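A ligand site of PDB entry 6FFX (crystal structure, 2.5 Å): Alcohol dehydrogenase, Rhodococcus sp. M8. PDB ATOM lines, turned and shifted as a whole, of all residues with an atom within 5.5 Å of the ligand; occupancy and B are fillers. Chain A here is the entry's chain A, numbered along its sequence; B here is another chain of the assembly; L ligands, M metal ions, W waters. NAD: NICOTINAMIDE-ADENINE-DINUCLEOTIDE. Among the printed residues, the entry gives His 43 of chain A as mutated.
N of Ile 271 lies within hydrogen-bond range of O3D of the ligand.
The guanidinium group of Arg 340 is in salt-bridge range of an oxygen (O1N) of the ligand (2.7 Å).
OG of Ser 223 lies within hydrogen-bond range of N1A of the ligand (3.0 Å).
The backbone carbonyl oxygen (O) of Pro 293 sits at hydrogen-bond distance from a nitrogen (N7N) of the ligand, at 3.2 Å.
The backbone NH of Gly 182 lies within hydrogen-bond range of an oxygen (O2A) of the ligand.
An oxygen (O2D) of the ligand is in hydrogen-bond range of a ring nitrogen (NE2) of His 43, 3.1 Å away.
O1A of the ligand is in hydrogen-bond range of ND1 of His 39 (2.9 Å).
O2B of the ligand lies within hydrogen-bond range of OD1 of Asp 203, 2.7 Å away.
An oxygen (O3B) of the ligand is in hydrogen-bond range of the backbone carbonyl oxygen (O) of Val 180.
N of His 39 lies close to O1N of the ligand (3.4 Å).
The side-chain hydroxyl (OG) of Ser 40 lies within hydrogen-bond range of an oxygen (O2D) of the ligand (2.8 Å).
O3B of the ligand is in hydrogen-bond range of NH1 of Arg 208, 2.7 Å away.
The backbone NH (N) of Leu 183 lies within hydrogen-bond range of an oxygen (O2N) of the ligand.
N of Trp 295 is in hydrogen-bond range of O7N of the ligand (3.1 Å).
O of Val 269 sits close to N7N of the ligand, 3.4 Å away.
The backbone NH (N) of Gly 179 is in hydrogen-bond range of the backbone carbonyl oxygen (O) of Val 202, 2.7 Å away.
The side-chain hydroxyl (OG1) of Thr 252 lies within hydrogen-bond range of the backbone carbonyl oxygen (O) of Ala 249, at 2.7 Å.
The side-chain carboxylate (OD1) of Asp 153 is in hydrogen-bond range of the side-chain hydroxyl (OG1) of Thr 157 (2.7 Å).
The backbone NH (N) of Ser 223 lies within hydrogen-bond range of the backbone carbonyl oxygen (O) of Asp 203 (2.9 Å).
The backbone NH of Asp 205 is in hydrogen-bond range of the side-chain carboxylate of Asp 203, 3.1 Å away.
OD2 of Asp 203 sits at hydrogen-bond distance from N of Val 180 (2.7 Å).
The backbone NH of Ser 40 sits close to the side-chain sulfur of Cys 38 (3.5 Å).
NH2 of Arg 340 lies close to SG of Cys 38 (3.0 Å).
Cys 38 touches the ligand (SG to C6N, 3.8 Å).
OD1 of Asp 153 touches C5N of the ligand, at 3.2 Å.
Thr 157 touches the ligand (OG1 to C4N, 3.4 Å).
Ile 178 touches the ligand (CG2 to C2A, 3.9 Å).
Gly 179 touches the ligand (CA to O4B, 3.8 Å).
CA of Gly 181 touches O5B of the ligand, at 3.2 Å.
Leu 204 touches the ligand.
Phe 246 touches the ligand.
Val 247 touches the ligand.
Thr 252 touches the ligand (CG2 to N1A, 3.6 Å).
CA of Gly 270 touches O4D of the ligand (3.8 Å).
CD1 of Tyr 294 touches O7N of the ligand, 3.6 Å away.
Phe 281 of chain B touches the ligand.
Hydrophobic or aromatic side chains that line the ligand: His 39, His 43, Ile 178, Leu 183, Leu 204, Val 247, Val 269, Ile 271, Tyr 294 and Phe 281 of chain B.
Within 4 Å of the ligand: Cys 38, His 39, Ser 40, His 43, Asp 153, Thr 157, Ile 178, Gly 179, Val 180, Gly 181, Gly 182, Leu 183, Asp 203, Leu 204, Arg 208, Ser 223, Phe 246, Val 247, Thr 252, Val 269, Gly 270, Ile 271, Pro 293, Tyr 294, Trp 295, Arg 340 and Phe 281 of chain B.
Water W2 bridges O of Val 247 (2.7 Å) and O3D of the ligand (2.9 Å).
Water W1 lies within hydrogen-bond range of O2N of the ligand (3.0 Å), O of Gly 179 (3.1 Å), N of Gly 181 (3.2 Å) and N of Gly 184 (3.3 Å).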
ATOM      1  N   CYS A  38     -20.698  30.841 -24.156  1.00  0.00           N
ATOM      2  CA  CYS A  38     -19.534  29.982 -24.079  1.00  0.00           C
ATOM      3  C   CYS A  38     -18.898  30.033 -22.687  1.00  0.00           C
ATOM      4  O   CYS A  38     -18.999  31.052 -22.001  1.00  0.00           O
ATOM      5  CB  CYS A  38     -18.512  30.373 -25.132  1.00  0.00           C
ATOM      6  SG  CYS A  38     -17.118  29.222 -25.182  1.00  0.00           S
ATOM      7  N   HIS A  39     -18.249  28.943 -22.285  1.00  0.00           N
ATOM      8  CA  HIS A  39     -17.567  28.886 -20.984  1.00  0.00           C
ATOM      9  C   HIS A  39     -16.465  29.960 -20.930  1.00  0.00           C
ATOM     10  O   HIS A  39     -16.192  30.502 -19.871  1.00  0.00           O
ATOM     11  CB  HIS A  39     -17.009  27.484 -20.694  1.00  0.00           C
ATOM     12  CG  HIS A  39     -16.821  27.187 -19.235  1.00  0.00           C
ATOM     13  ND1 HIS A  39     -17.793  26.562 -18.468  1.00  0.00           N
ATOM     14  CD2 HIS A  39     -15.784  27.425 -18.396  1.00  0.00           C
ATOM     15  CE1 HIS A  39     -17.337  26.411 -17.232  1.00  0.00           C
ATOM     16  NE2 HIS A  39     -16.128  26.936 -17.157  1.00  0.00           N
ATOM     17  N   SER A  40     -15.873  30.274 -22.078  1.00  0.00           N
ATOM     18  CA  SER A  40     -14.897  31.356 -22.166  1.00  0.00           C
ATOM     19  C   SER A  40     -15.400  32.739 -21.729  1.00  0.00           C
ATOM     20  O   SER A  40     -14.607  33.551 -21.268  1.00  0.00           O
ATOM     21  CB  SER A  40     -14.290  31.441 -23.565  1.00  0.00           C
ATOM     22  OG  SER A  40     -13.482  30.295 -23.811  1.00  0.00           O
ATOM     23  N   HIS A  43     -14.488  32.990 -18.019  1.00  0.00           N
ATOM     24  CA  HIS A  43     -13.064  33.345 -17.818  1.00  0.00           C
ATOM     25  C   HIS A  43     -12.877  34.846 -17.950  1.00  0.00           C
ATOM     26  O   HIS A  43     -12.159  35.446 -17.141  1.00  0.00           O
ATOM     27  CB  HIS A  43     -12.099  32.639 -18.817  1.00  0.00           C
ATOM     28  CG  HIS A  43     -12.112  31.126 -18.727  1.00  0.00           C
ATOM     29  ND1 HIS A  43     -12.278  30.446 -17.544  1.00  0.00           N
ATOM     30  CD2 HIS A  43     -11.977  30.180 -19.691  1.00  0.00           C
ATOM     31  CE1 HIS A  43     -12.314  29.156 -17.774  1.00  0.00           C
ATOM     32  NE2 HIS A  43     -12.124  28.961 -19.073  1.00  0.00           N
ATOM     33  N   ASP A 153     -18.258  28.496 -32.543  1.00  0.00           N
ATOM     34  CA  ASP A 153     -17.204  28.282 -31.568  1.00  0.00           C
ATOM     35  C   ASP A 153     -17.213  26.842 -31.020  1.00  0.00           C
ATOM     36  O   ASP A 153     -16.206  26.116 -31.143  1.00  0.00           O
ATOM     37  CB  ASP A 153     -17.367  29.286 -30.428  1.00  0.00           C
ATOM     38  CG  ASP A 153     -16.196  29.311 -29.477  1.00  0.00           C
ATOM     39  OD1 ASP A 153     -15.175  28.616 -29.682  1.00  0.00           O
ATOM     40  OD2 ASP A 153     -16.347  30.049 -28.489  1.00  0.00           O
ATOM     41  N   THR A 157     -14.229  25.276 -32.821  1.00  0.00           N
ATOM     42  CA  THR A 157     -13.020  25.046 -32.031  1.00  0.00           C
ATOM     43  C   THR A 157     -12.607  23.554 -32.011  1.00  0.00           C
ATOM     44  O   THR A 157     -11.446  23.257 -32.274  1.00  0.00           O
ATOM     45  CB  THR A 157     -13.134  25.615 -30.623  1.00  0.00           C
ATOM     46  OG1 THR A 157     -13.259  27.028 -30.705  1.00  0.00           O
ATOM     47  CG2 THR A 157     -11.949  25.270 -29.785  1.00  0.00           C
ATOM     48  N   ILE A 178     -12.046  14.246 -23.900  1.00  0.00           N
ATOM     49  CA  ILE A 178     -12.215  14.486 -22.466  1.00  0.00           C
ATOM     50  C   ILE A 178     -13.061  15.736 -22.261  1.00  0.00           C
ATOM     51  O   ILE A 178     -12.666  16.804 -22.675  1.00  0.00           O
ATOM     52  CB  ILE A 178     -10.887  14.628 -21.727  1.00  0.00           C
ATOM     53  CG1 ILE A 178      -9.967  13.441 -22.029  1.00  0.00           C
ATOM     54  CG2 ILE A 178     -11.110  14.732 -20.226  1.00  0.00           C
ATOM     55  CD1 ILE A 178      -8.568  13.564 -21.460  1.00  0.00           C
ATOM     56  N   GLY A 179     -14.209  15.593 -21.617  1.00  0.00           N
ATOM     57  CA  GLY A 179     -15.130  16.693 -21.358  1.00  0.00           C
ATOM     58  C   GLY A 179     -16.233  16.745 -22.404  1.00  0.00           C
ATOM     59  O   GLY A 179     -16.036  17.324 -23.469  1.00  0.00           O
ATOM     60  N   VAL A 180     -17.390  16.169 -22.098  1.00  0.00           N
ATOM     61  CA  VAL A 180     -18.531  16.082 -23.006  1.00  0.00           C
ATOM     62  C   VAL A 180     -19.537  17.198 -22.708  1.00  0.00           C
ATOM     63  O   VAL A 180     -20.691  16.955 -22.378  1.00  0.00           O
ATOM     64  CB  VAL A 180     -19.174  14.683 -22.954  1.00  0.00           C
ATOM     65  CG1 VAL A 180     -20.192  14.509 -24.066  1.00  0.00           C
ATOM     66  CG2 VAL A 180     -18.094  13.617 -23.122  1.00  0.00           C
ATOM     67  N   GLY A 181     -19.059  18.436 -22.832  1.00  0.00           N
ATOM     68  CA  GLY A 181     -19.873  19.624 -22.584  1.00  0.00           C
ATOM     69  C   GLY A 181     -20.229  20.237 -23.910  1.00  0.00           C
ATOM     70  O   GLY A 181     -20.423  19.519 -24.906  1.00  0.00           O
ATOM     71  N   GLY A 182     -20.312  21.575 -23.939  1.00  0.00           N
ATOM     72  CA  GLY A 182     -20.651  22.295 -25.160  1.00  0.00           C
ATOM     73  C   GLY A 182     -19.777  21.872 -26.318  1.00  0.00           C
ATOM     74  O   GLY A 182     -20.291  21.432 -27.350  1.00  0.00           O
ATOM     75  N   LEU A 183     -18.464  21.924 -26.116  1.00  0.00           N
ATOM     76  CA  LEU A 183     -17.515  21.615 -27.160  1.00  0.00           C
ATOM     77  C   LEU A 183     -17.418  20.125 -27.452  1.00  0.00           C
ATOM     78  O   LEU A 183     -17.493  19.673 -28.617  1.00  0.00           O
ATOM     79  CB  LEU A 183     -16.127  22.168 -26.828  1.00  0.00           C
ATOM     80  CG  LEU A 183     -15.805  23.576 -27.318  1.00  0.00           C
ATOM     81  CD1 LEU A 183     -16.705  24.606 -26.689  1.00  0.00           C
ATOM     82  CD2 LEU A 183     -14.374  23.944 -27.022  1.00  0.00           C
ATOM     83  N   GLY A 184     -17.257  19.350 -26.397  1.00  0.00           N
ATOM     84  CA  GLY A 184     -16.920  17.944 -26.508  1.00  0.00           C
ATOM     85  C   GLY A 184     -17.982  17.084 -27.154  1.00  0.00           C
ATOM     86  O   GLY A 184     -17.660  16.156 -27.879  1.00  0.00           O
ATOM     87  N   VAL A 202     -14.754  10.832 -22.197  1.00  0.00           N
ATOM     88  CA  VAL A 202     -14.402  10.853 -20.766  1.00  0.00           C
ATOM     89  C   VAL A 202     -15.037  12.060 -20.118  1.00  0.00           C
ATOM     90  O   VAL A 202     -14.925  13.161 -20.631  1.00  0.00           O
ATOM     91  CB  VAL A 202     -12.882  10.899 -20.543  1.00  0.00           C
ATOM     92  CG1 VAL A 202     -12.542  10.733 -19.052  1.00  0.00           C
ATOM     93  CG2 VAL A 202     -12.173   9.860 -21.380  1.00  0.00           C
ATOM     94  N   ASP A 203     -15.716  11.845 -18.992  1.00  0.00           N
ATOM     95  CA  ASP A 203     -16.350  12.931 -18.236  1.00  0.00           C
ATOM     96  C   ASP A 203     -16.532  12.510 -16.802  1.00  0.00           C
ATOM     97  O   ASP A 203     -16.510  11.322 -16.520  1.00  0.00           O
ATOM     98  CB  ASP A 203     -17.687  13.322 -18.875  1.00  0.00           C
ATOM     99  CG  ASP A 203     -18.086  14.757 -18.591  1.00  0.00           C
ATOM    100  OD1 ASP A 203     -18.359  15.089 -17.414  1.00  0.00           O
ATOM    101  OD2 ASP A 203     -18.126  15.535 -19.539  1.00  0.00           O
ATOM    102  N   LEU A 204     -16.663  13.489 -15.908  1.00  0.00           N
ATOM    103  CA  LEU A 204     -16.969  13.212 -14.483  1.00  0.00           C
ATOM    104  C   LEU A 204     -18.424  12.811 -14.242  1.00  0.00           C
ATOM    105  O   LEU A 204     -18.721  11.985 -13.385  1.00  0.00           O
ATOM    106  CB  LEU A 204     -16.698  14.458 -13.623  1.00  0.00           C
ATOM    107  CG  LEU A 204     -15.223  14.799 -13.395  1.00  0.00           C
ATOM    108  CD1 LEU A 204     -15.153  16.216 -12.810  1.00  0.00           C
ATOM    109  CD2 LEU A 204     -14.549  13.795 -12.468  1.00  0.00           C
ATOM    110  N   ASP A 205     -19.324  13.417 -15.002  1.00  0.00           N
ATOM    111  CA  ASP A 205     -20.773  13.284 -14.866  1.00  0.00           C
ATOM    112  C   ASP A 205     -21.304  12.122 -15.735  1.00  0.00           C
ATOM    113  O   ASP A 205     -21.124  12.102 -16.950  1.00  0.00           O
ATOM    114  CB  ASP A 205     -21.390  14.613 -15.306  1.00  0.00           C
ATOM    115  CG  ASP A 205     -22.864  14.745 -14.991  1.00  0.00           C
ATOM    116  OD1 ASP A 205     -23.545  13.728 -14.757  1.00  0.00           O
ATOM    117  OD2 ASP A 205     -23.349  15.880 -15.001  1.00  0.00           O
ATOM    118  N   ARG A 208     -23.403  13.121 -18.651  1.00  0.00           N
ATOM    119  CA  ARG A 208     -22.619  13.547 -19.804  1.00  0.00           C
ATOM    120  C   ARG A 208     -22.030  12.352 -20.557  1.00  0.00           C
ATOM    121  O   ARG A 208     -21.888  12.401 -21.766  1.00  0.00           O
ATOM    122  CB  ARG A 208     -21.536  14.536 -19.380  1.00  0.00           C
ATOM    123  CG  ARG A 208     -22.054  15.815 -18.769  1.00  0.00           C
ATOM    124  CD  ARG A 208     -22.909  16.660 -19.716  1.00  0.00           C
ATOM    125  NE  ARG A 208     -23.516  17.801 -19.009  1.00  0.00           N
ATOM    126  CZ  ARG A 208     -23.013  19.040 -18.946  1.00  0.00           C
ATOM    127  NH1 ARG A 208     -21.902  19.388 -19.571  1.00  0.00           N
ATOM    128  NH2 ARG A 208     -23.673  19.965 -18.261  1.00  0.00           N
ATOM    129  N   SER A 223     -14.112   9.987 -15.568  1.00  0.00           N
ATOM    130  CA  SER A 223     -12.829  10.669 -15.364  1.00  0.00           C
ATOM    131  C   SER A 223     -12.320  10.491 -13.928  1.00  0.00           C
ATOM    132  O   SER A 223     -13.059  10.073 -13.011  1.00  0.00           O
ATOM    133  CB  SER A 223     -12.936  12.173 -15.688  1.00  0.00           C
ATOM    134  OG  SER A 223     -11.675  12.718 -16.033  1.00  0.00           O
ATOM    135  N   PHE A 246     -10.991  18.785 -23.749  1.00  0.00           N
ATOM    136  CA  PHE A 246     -11.800  20.007 -23.693  1.00  0.00           C
ATOM    137  C   PHE A 246     -11.998  20.529 -22.283  1.00  0.00           C
ATOM    138  O   PHE A 246     -12.710  21.513 -22.093  1.00  0.00           O
ATOM    139  CB  PHE A 246     -13.149  19.780 -24.370  1.00  0.00           C
ATOM    140  CG  PHE A 246     -13.016  19.452 -25.818  1.00  0.00           C
ATOM    141  CD1 PHE A 246     -12.798  20.442 -26.754  1.00  0.00           C
ATOM    142  CD2 PHE A 246     -13.094  18.128 -26.259  1.00  0.00           C
ATOM    143  CE1 PHE A 246     -12.658  20.147 -28.086  1.00  0.00           C
ATOM    144  CE2 PHE A 246     -12.971  17.819 -27.591  1.00  0.00           C
ATOM    145  CZ  PHE A 246     -12.757  18.819 -28.495  1.00  0.00           C
ATOM    146  N   VAL A 247     -11.371  19.890 -21.307  1.00  0.00           N
ATOM    147  CA  VAL A 247     -11.409  20.346 -19.918  1.00  0.00           C
ATOM    148  C   VAL A 247     -10.138  21.138 -19.651  1.00  0.00           C
ATOM    149  O   VAL A 247     -10.198  22.275 -19.179  1.00  0.00           O
ATOM    150  CB  VAL A 247     -11.469  19.167 -18.933  1.00  0.00           C
ATOM    151  CG1 VAL A 247     -11.597  19.672 -17.481  1.00  0.00           C
ATOM    152  CG2 VAL A 247     -12.615  18.228 -19.282  1.00  0.00           C
ATOM    153  N   ALA A 249      -7.714  20.733 -17.479  1.00  0.00           N
ATOM    154  CA  ALA A 249      -7.173  20.753 -16.126  1.00  0.00           C
ATOM    155  C   ALA A 249      -5.951  19.884 -16.093  1.00  0.00           C
ATOM    156  O   ALA A 249      -5.717  19.076 -17.006  1.00  0.00           O
ATOM    157  CB  ALA A 249      -8.195  20.245 -15.116  1.00  0.00           C
ATOM    158  N   SER A 251      -5.259  17.355 -14.220  1.00  0.00           N
ATOM    159  CA  SER A 251      -5.562  15.931 -14.091  1.00  0.00           C
ATOM    160  C   SER A 251      -5.981  15.316 -15.434  1.00  0.00           C
ATOM    161  O   SER A 251      -5.636  14.165 -15.718  1.00  0.00           O
ATOM    162  CB  SER A 251      -6.640  15.684 -13.019  1.00  0.00           C
ATOM    163  OG  SER A 251      -7.878  16.276 -13.381  1.00  0.00           O
ATOM    164  N   THR A 252      -6.693  16.078 -16.252  1.00  0.00           N
ATOM    165  CA  THR A 252      -7.096  15.620 -17.589  1.00  0.00           C
ATOM    166  C   THR A 252      -5.901  15.569 -18.541  1.00  0.00           C
ATOM    167  O   THR A 252      -5.779  14.659 -19.350  1.00  0.00           O
ATOM    168  CB  THR A 252      -8.195  16.496 -18.204  1.00  0.00           C
ATOM    169  OG1 THR A 252      -7.762  17.862 -18.267  1.00  0.00           O
ATOM    170  CG2 THR A 252      -9.473  16.387 -17.377  1.00  0.00           C
ATOM    171  N   VAL A 269      -7.409  21.786 -25.387  1.00  0.00           N
ATOM    172  CA  VAL A 269      -8.367  22.792 -25.875  1.00  0.00           C
ATOM    173  C   VAL A 269      -9.025  23.553 -24.735  1.00  0.00           C
ATOM    174  O   VAL A 269      -9.216  24.752 -24.842  1.00  0.00           O
ATOM    175  CB  VAL A 269      -9.439  22.148 -26.755  1.00  0.00           C
ATOM    176  CG1 VAL A 269     -10.421  23.190 -27.235  1.00  0.00           C
ATOM    177  CG2 VAL A 269      -8.754  21.456 -27.929  1.00  0.00           C
ATOM    178  N   GLY A 270      -9.369  22.857 -23.674  1.00  0.00           N
ATOM    179  CA  GLY A 270      -9.835  23.500 -22.468  1.00  0.00           C
ATOM    180  C   GLY A 270      -8.742  24.306 -21.773  1.00  0.00           C
ATOM    181  O   GLY A 270      -7.554  24.022 -21.888  1.00  0.00           O
ATOM    182  N   ILE A 271      -9.184  25.314 -21.027  1.00  0.00           N
ATOM    183  CA  ILE A 271      -8.312  26.333 -20.456  1.00  0.00           C
ATOM    184  C   ILE A 271      -8.422  26.325 -18.935  1.00  0.00           C
ATOM    185  O   ILE A 271      -9.431  26.683 -18.390  1.00  0.00           O
ATOM    186  CB  ILE A 271      -8.704  27.720 -21.027  1.00  0.00           C
ATOM    187  CG1 ILE A 271      -8.514  27.728 -22.548  1.00  0.00           C
ATOM    188  CG2 ILE A 271      -7.904  28.828 -20.362  1.00  0.00           C
ATOM    189  CD1 ILE A 271      -9.029  28.943 -23.273  1.00  0.00           C
ATOM    190  N   PRO A 293      -4.537  24.531 -29.360  1.00  0.00           N
ATOM    191  CA  PRO A 293      -5.066  25.258 -30.495  1.00  0.00           C
ATOM    192  C   PRO A 293      -6.009  26.380 -30.055  1.00  0.00           C
ATOM    193  O   PRO A 293      -6.416  26.425 -28.891  1.00  0.00           O
ATOM    194  CB  PRO A 293      -5.823  24.196 -31.267  1.00  0.00           C
ATOM    195  CG  PRO A 293      -6.272  23.234 -30.238  1.00  0.00           C
ATOM    196  CD  PRO A 293      -5.388  23.375 -29.030  1.00  0.00           C
ATOM    197  N   TYR A 294      -6.292  27.303 -30.960  1.00  0.00           N
ATOM    198  CA  TYR A 294      -7.152  28.446 -30.672  1.00  0.00           C
ATOM    199  C   TYR A 294      -8.226  28.586 -31.783  1.00  0.00           C
ATOM    200  O   TYR A 294      -7.900  28.734 -32.972  1.00  0.00           O
ATOM    201  CB  TYR A 294      -6.326  29.716 -30.541  1.00  0.00           C
ATOM    202  CG  TYR A 294      -7.112  31.010 -30.495  1.00  0.00           C
ATOM    203  CD1 TYR A 294      -7.863  31.356 -29.374  1.00  0.00           C
ATOM    204  CD2 TYR A 294      -7.087  31.911 -31.553  1.00  0.00           C
ATOM    205  CE1 TYR A 294      -8.551  32.578 -29.302  1.00  0.00           C
ATOM    206  CE2 TYR A 294      -7.771  33.123 -31.513  1.00  0.00           C
ATOM    207  CZ  TYR A 294      -8.503  33.459 -30.384  1.00  0.00           C
ATOM    208  OH  TYR A 294      -9.208  34.647 -30.336  1.00  0.00           O
ATOM    209  N   TRP A 295      -9.483  28.492 -31.372  1.00  0.00           N
ATOM    210  CA  TRP A 295     -10.624  28.769 -32.202  1.00  0.00           C
ATOM    211  C   TRP A 295     -10.493  28.013 -33.538  1.00  0.00           C
ATOM    212  O   TRP A 295     -10.243  26.831 -33.499  1.00  0.00           O
ATOM    213  CB  TRP A 295     -10.823  30.288 -32.326  1.00  0.00           C
ATOM    214  CG  TRP A 295     -12.255  30.726 -32.311  1.00  0.00           C
ATOM    215  CD1 TRP A 295     -13.345  30.031 -32.783  1.00  0.00           C
ATOM    216  CD2 TRP A 295     -12.767  31.969 -31.815  1.00  0.00           C
ATOM    217  NE1 TRP A 295     -14.494  30.763 -32.599  1.00  0.00           N
ATOM    218  CE2 TRP A 295     -14.162  31.959 -32.003  1.00  0.00           C
ATOM    219  CE3 TRP A 295     -12.185  33.094 -31.220  1.00  0.00           C
ATOM    220  CZ2 TRP A 295     -14.979  33.031 -31.624  1.00  0.00           C
ATOM    221  CZ3 TRP A 295     -13.002  34.159 -30.849  1.00  0.00           C
ATOM    222  CH2 TRP A 295     -14.374  34.113 -31.045  1.00  0.00           C
ATOM    223  N   LEU A 332     -24.707  28.472 -16.464  1.00  0.00           N
ATOM    224  CA  LEU A 332     -23.469  27.975 -17.085  1.00  0.00           C
ATOM    225  C   LEU A 332     -22.333  27.764 -16.072  1.00  0.00           C
ATOM    226  O   LEU A 332     -21.545  26.828 -16.223  1.00  0.00           O
ATOM    227  CB  LEU A 332     -23.022  28.903 -18.219  1.00  0.00           C
ATOM    228  CG  LEU A 332     -21.814  28.479 -19.079  1.00  0.00           C
ATOM    229  CD1 LEU A 332     -21.931  27.052 -19.616  1.00  0.00           C
ATOM    230  CD2 LEU A 332     -21.634  29.470 -20.204  1.00  0.00           C
ATOM    231  N   GLY A 339     -25.471  20.794 -22.819  1.00  0.00           N
ATOM    232  CA  GLY A 339     -25.009  21.173 -24.146  1.00  0.00           C
ATOM    233  C   GLY A 339     -24.604  22.634 -24.147  1.00  0.00           C
ATOM    234  O   GLY A 339     -23.711  23.052 -23.416  1.00  0.00           O
ATOM    235  N   ARG A 340     -25.278  23.427 -24.980  1.00  0.00           N
ATOM    236  CA  ARG A 340     -24.958  24.841 -25.168  1.00  0.00           C
ATOM    237  C   ARG A 340     -26.166  25.734 -24.927  1.00  0.00           C
ATOM    238  O   ARG A 340     -27.267  25.445 -25.386  1.00  0.00           O
ATOM    239  CB  ARG A 340     -24.438  25.062 -26.582  1.00  0.00           C
ATOM    240  CG  ARG A 340     -23.683  26.380 -26.735  1.00  0.00           C
ATOM    241  CD  ARG A 340     -22.470  26.430 -25.860  1.00  0.00           C
ATOM    242  NE  ARG A 340     -21.301  27.095 -26.459  1.00  0.00           N
ATOM    243  CZ  ARG A 340     -20.045  26.861 -26.095  1.00  0.00           C
ATOM    244  NH1 ARG A 340     -19.744  26.012 -25.122  1.00  0.00           N
ATOM    245  NH2 ARG A 340     -19.054  27.517 -26.688  1.00  0.00           N
ATOM    246  N   PHE B 281      -2.084  26.928 -21.981  1.00  0.00           N
ATOM    247  CA  PHE B 281      -2.472  28.299 -22.348  1.00  0.00           C
ATOM    248  C   PHE B 281      -1.710  29.295 -21.517  1.00  0.00           C
ATOM    249  O   PHE B 281      -1.431  29.032 -20.356  1.00  0.00           O
ATOM    250  CB  PHE B 281      -3.989  28.506 -22.275  1.00  0.00           C
ATOM    251  CG  PHE B 281      -4.730  27.731 -23.344  1.00  0.00           C
ATOM    252  CD1 PHE B 281      -4.901  28.256 -24.618  1.00  0.00           C
ATOM    253  CD2 PHE B 281      -5.178  26.441 -23.080  1.00  0.00           C
ATOM    254  CE1 PHE B 281      -5.547  27.523 -25.603  1.00  0.00           C
ATOM    255  CE2 PHE B 281      -5.833  25.704 -24.062  1.00  0.00           C
ATOM    256  CZ  PHE B 281      -6.039  26.244 -25.322  1.00  0.00           C
HETATM  257  PA  NAD L   1     -18.970  23.342 -20.709  1.00  0.00           P
HETATM  258  O1A NAD L   1     -19.034  24.094 -19.384  1.00  0.00           O
HETATM  259  O2A NAD L   1     -20.039  23.536 -21.747  1.00  0.00           O
HETATM  260  O5B NAD L   1     -18.812  21.771 -20.418  1.00  0.00           O
HETATM  261  C5B NAD L   1     -17.837  21.269 -19.521  1.00  0.00           C
HETATM  262  C4B NAD L   1     -17.839  19.740 -19.511  1.00  0.00           C
HETATM  263  O4B NAD L   1     -16.581  19.306 -19.008  1.00  0.00           O
HETATM  264  C3B NAD L   1     -18.911  19.143 -18.609  1.00  0.00           C
HETATM  265  O3B NAD L   1     -19.558  18.038 -19.263  1.00  0.00           O
HETATM  266  C2B NAD L   1     -18.163  18.699 -17.364  1.00  0.00           C
HETATM  267  O2B NAD L   1     -18.770  17.598 -16.666  1.00  0.00           O
HETATM  268  C1B NAD L   1     -16.793  18.356 -17.947  1.00  0.00           C
HETATM  269  N9A NAD L   1     -15.695  18.290 -16.930  1.00  0.00           N
HETATM  270  C8A NAD L   1     -15.401  19.177 -15.937  1.00  0.00           C
HETATM  271  N7A NAD L   1     -14.331  18.739 -15.205  1.00  0.00           N
HETATM  272  C5A NAD L   1     -13.940  17.554 -15.739  1.00  0.00           C
HETATM  273  C6A NAD L   1     -12.887  16.530 -15.475  1.00  0.00           C
HETATM  274  N6A NAD L   1     -12.010  16.670 -14.469  1.00  0.00           N
HETATM  275  N1A NAD L   1     -12.818  15.437 -16.268  1.00  0.00           N
HETATM  276  C2A NAD L   1     -13.685  15.250 -17.300  1.00  0.00           C
HETATM  277  N3A NAD L   1     -14.674  16.121 -17.601  1.00  0.00           N
HETATM  278  C4A NAD L   1     -14.846  17.259 -16.876  1.00  0.00           C
HETATM  279  O3  NAD L   1     -17.559  23.648 -21.416  1.00  0.00           O
HETATM  280  PN  NAD L   1     -17.376  24.303 -22.884  1.00  0.00           P
HETATM  281  O1N NAD L   1     -18.154  25.591 -23.006  1.00  0.00           O
HETATM  282  O2N NAD L   1     -17.535  23.160 -23.848  1.00  0.00           O
HETATM  283  O5D NAD L   1     -15.814  24.702 -22.909  1.00  0.00           O
HETATM  284  C5D NAD L   1     -14.833  23.851 -22.303  1.00  0.00           C
HETATM  285  C4D NAD L   1     -13.495  24.575 -22.271  1.00  0.00           C
HETATM  286  O4D NAD L   1     -13.123  24.936 -23.610  1.00  0.00           O
HETATM  287  C3D NAD L   1     -13.544  25.853 -21.428  1.00  0.00           C
HETATM  288  O3D NAD L   1     -12.453  25.864 -20.493  1.00  0.00           O
HETATM  289  C2D NAD L   1     -13.493  26.969 -22.477  1.00  0.00           C
HETATM  290  O2D NAD L   1     -12.924  28.193 -21.985  1.00  0.00           O
HETATM  291  C1D NAD L   1     -12.668  26.299 -23.591  1.00  0.00           C
HETATM  292  N1N NAD L   1     -12.741  26.879 -24.939  1.00  0.00           N
HETATM  293  C2N NAD L   1     -11.592  27.059 -25.629  1.00  0.00           C
HETATM  294  C3N NAD L   1     -11.566  27.606 -26.908  1.00  0.00           C
HETATM  295  C7N NAD L   1     -10.254  27.794 -27.644  1.00  0.00           C
HETATM  296  O7N NAD L   1     -10.138  28.769 -28.352  1.00  0.00           O
HETATM  297  N7N NAD L   1      -9.257  26.891 -27.542  1.00  0.00           N
HETATM  298  C4N NAD L   1     -12.775  27.980 -27.504  1.00  0.00           C
HETATM  299  C5N NAD L   1     -13.963  27.761 -26.807  1.00  0.00           C
HETATM  300  C6N NAD L   1     -13.925  27.214 -25.514  1.00  0.00           C
HETATM  301 ZN    ZN M   1     -15.804  30.646 -26.686  1.00  0.00          ZN
HETATM  302  O   HOH W   1     -16.584  20.368 -23.320  1.00  0.00           O
HETATM  303  O   HOH W   2     -12.300  23.782 -18.432  1.00  0.00           O
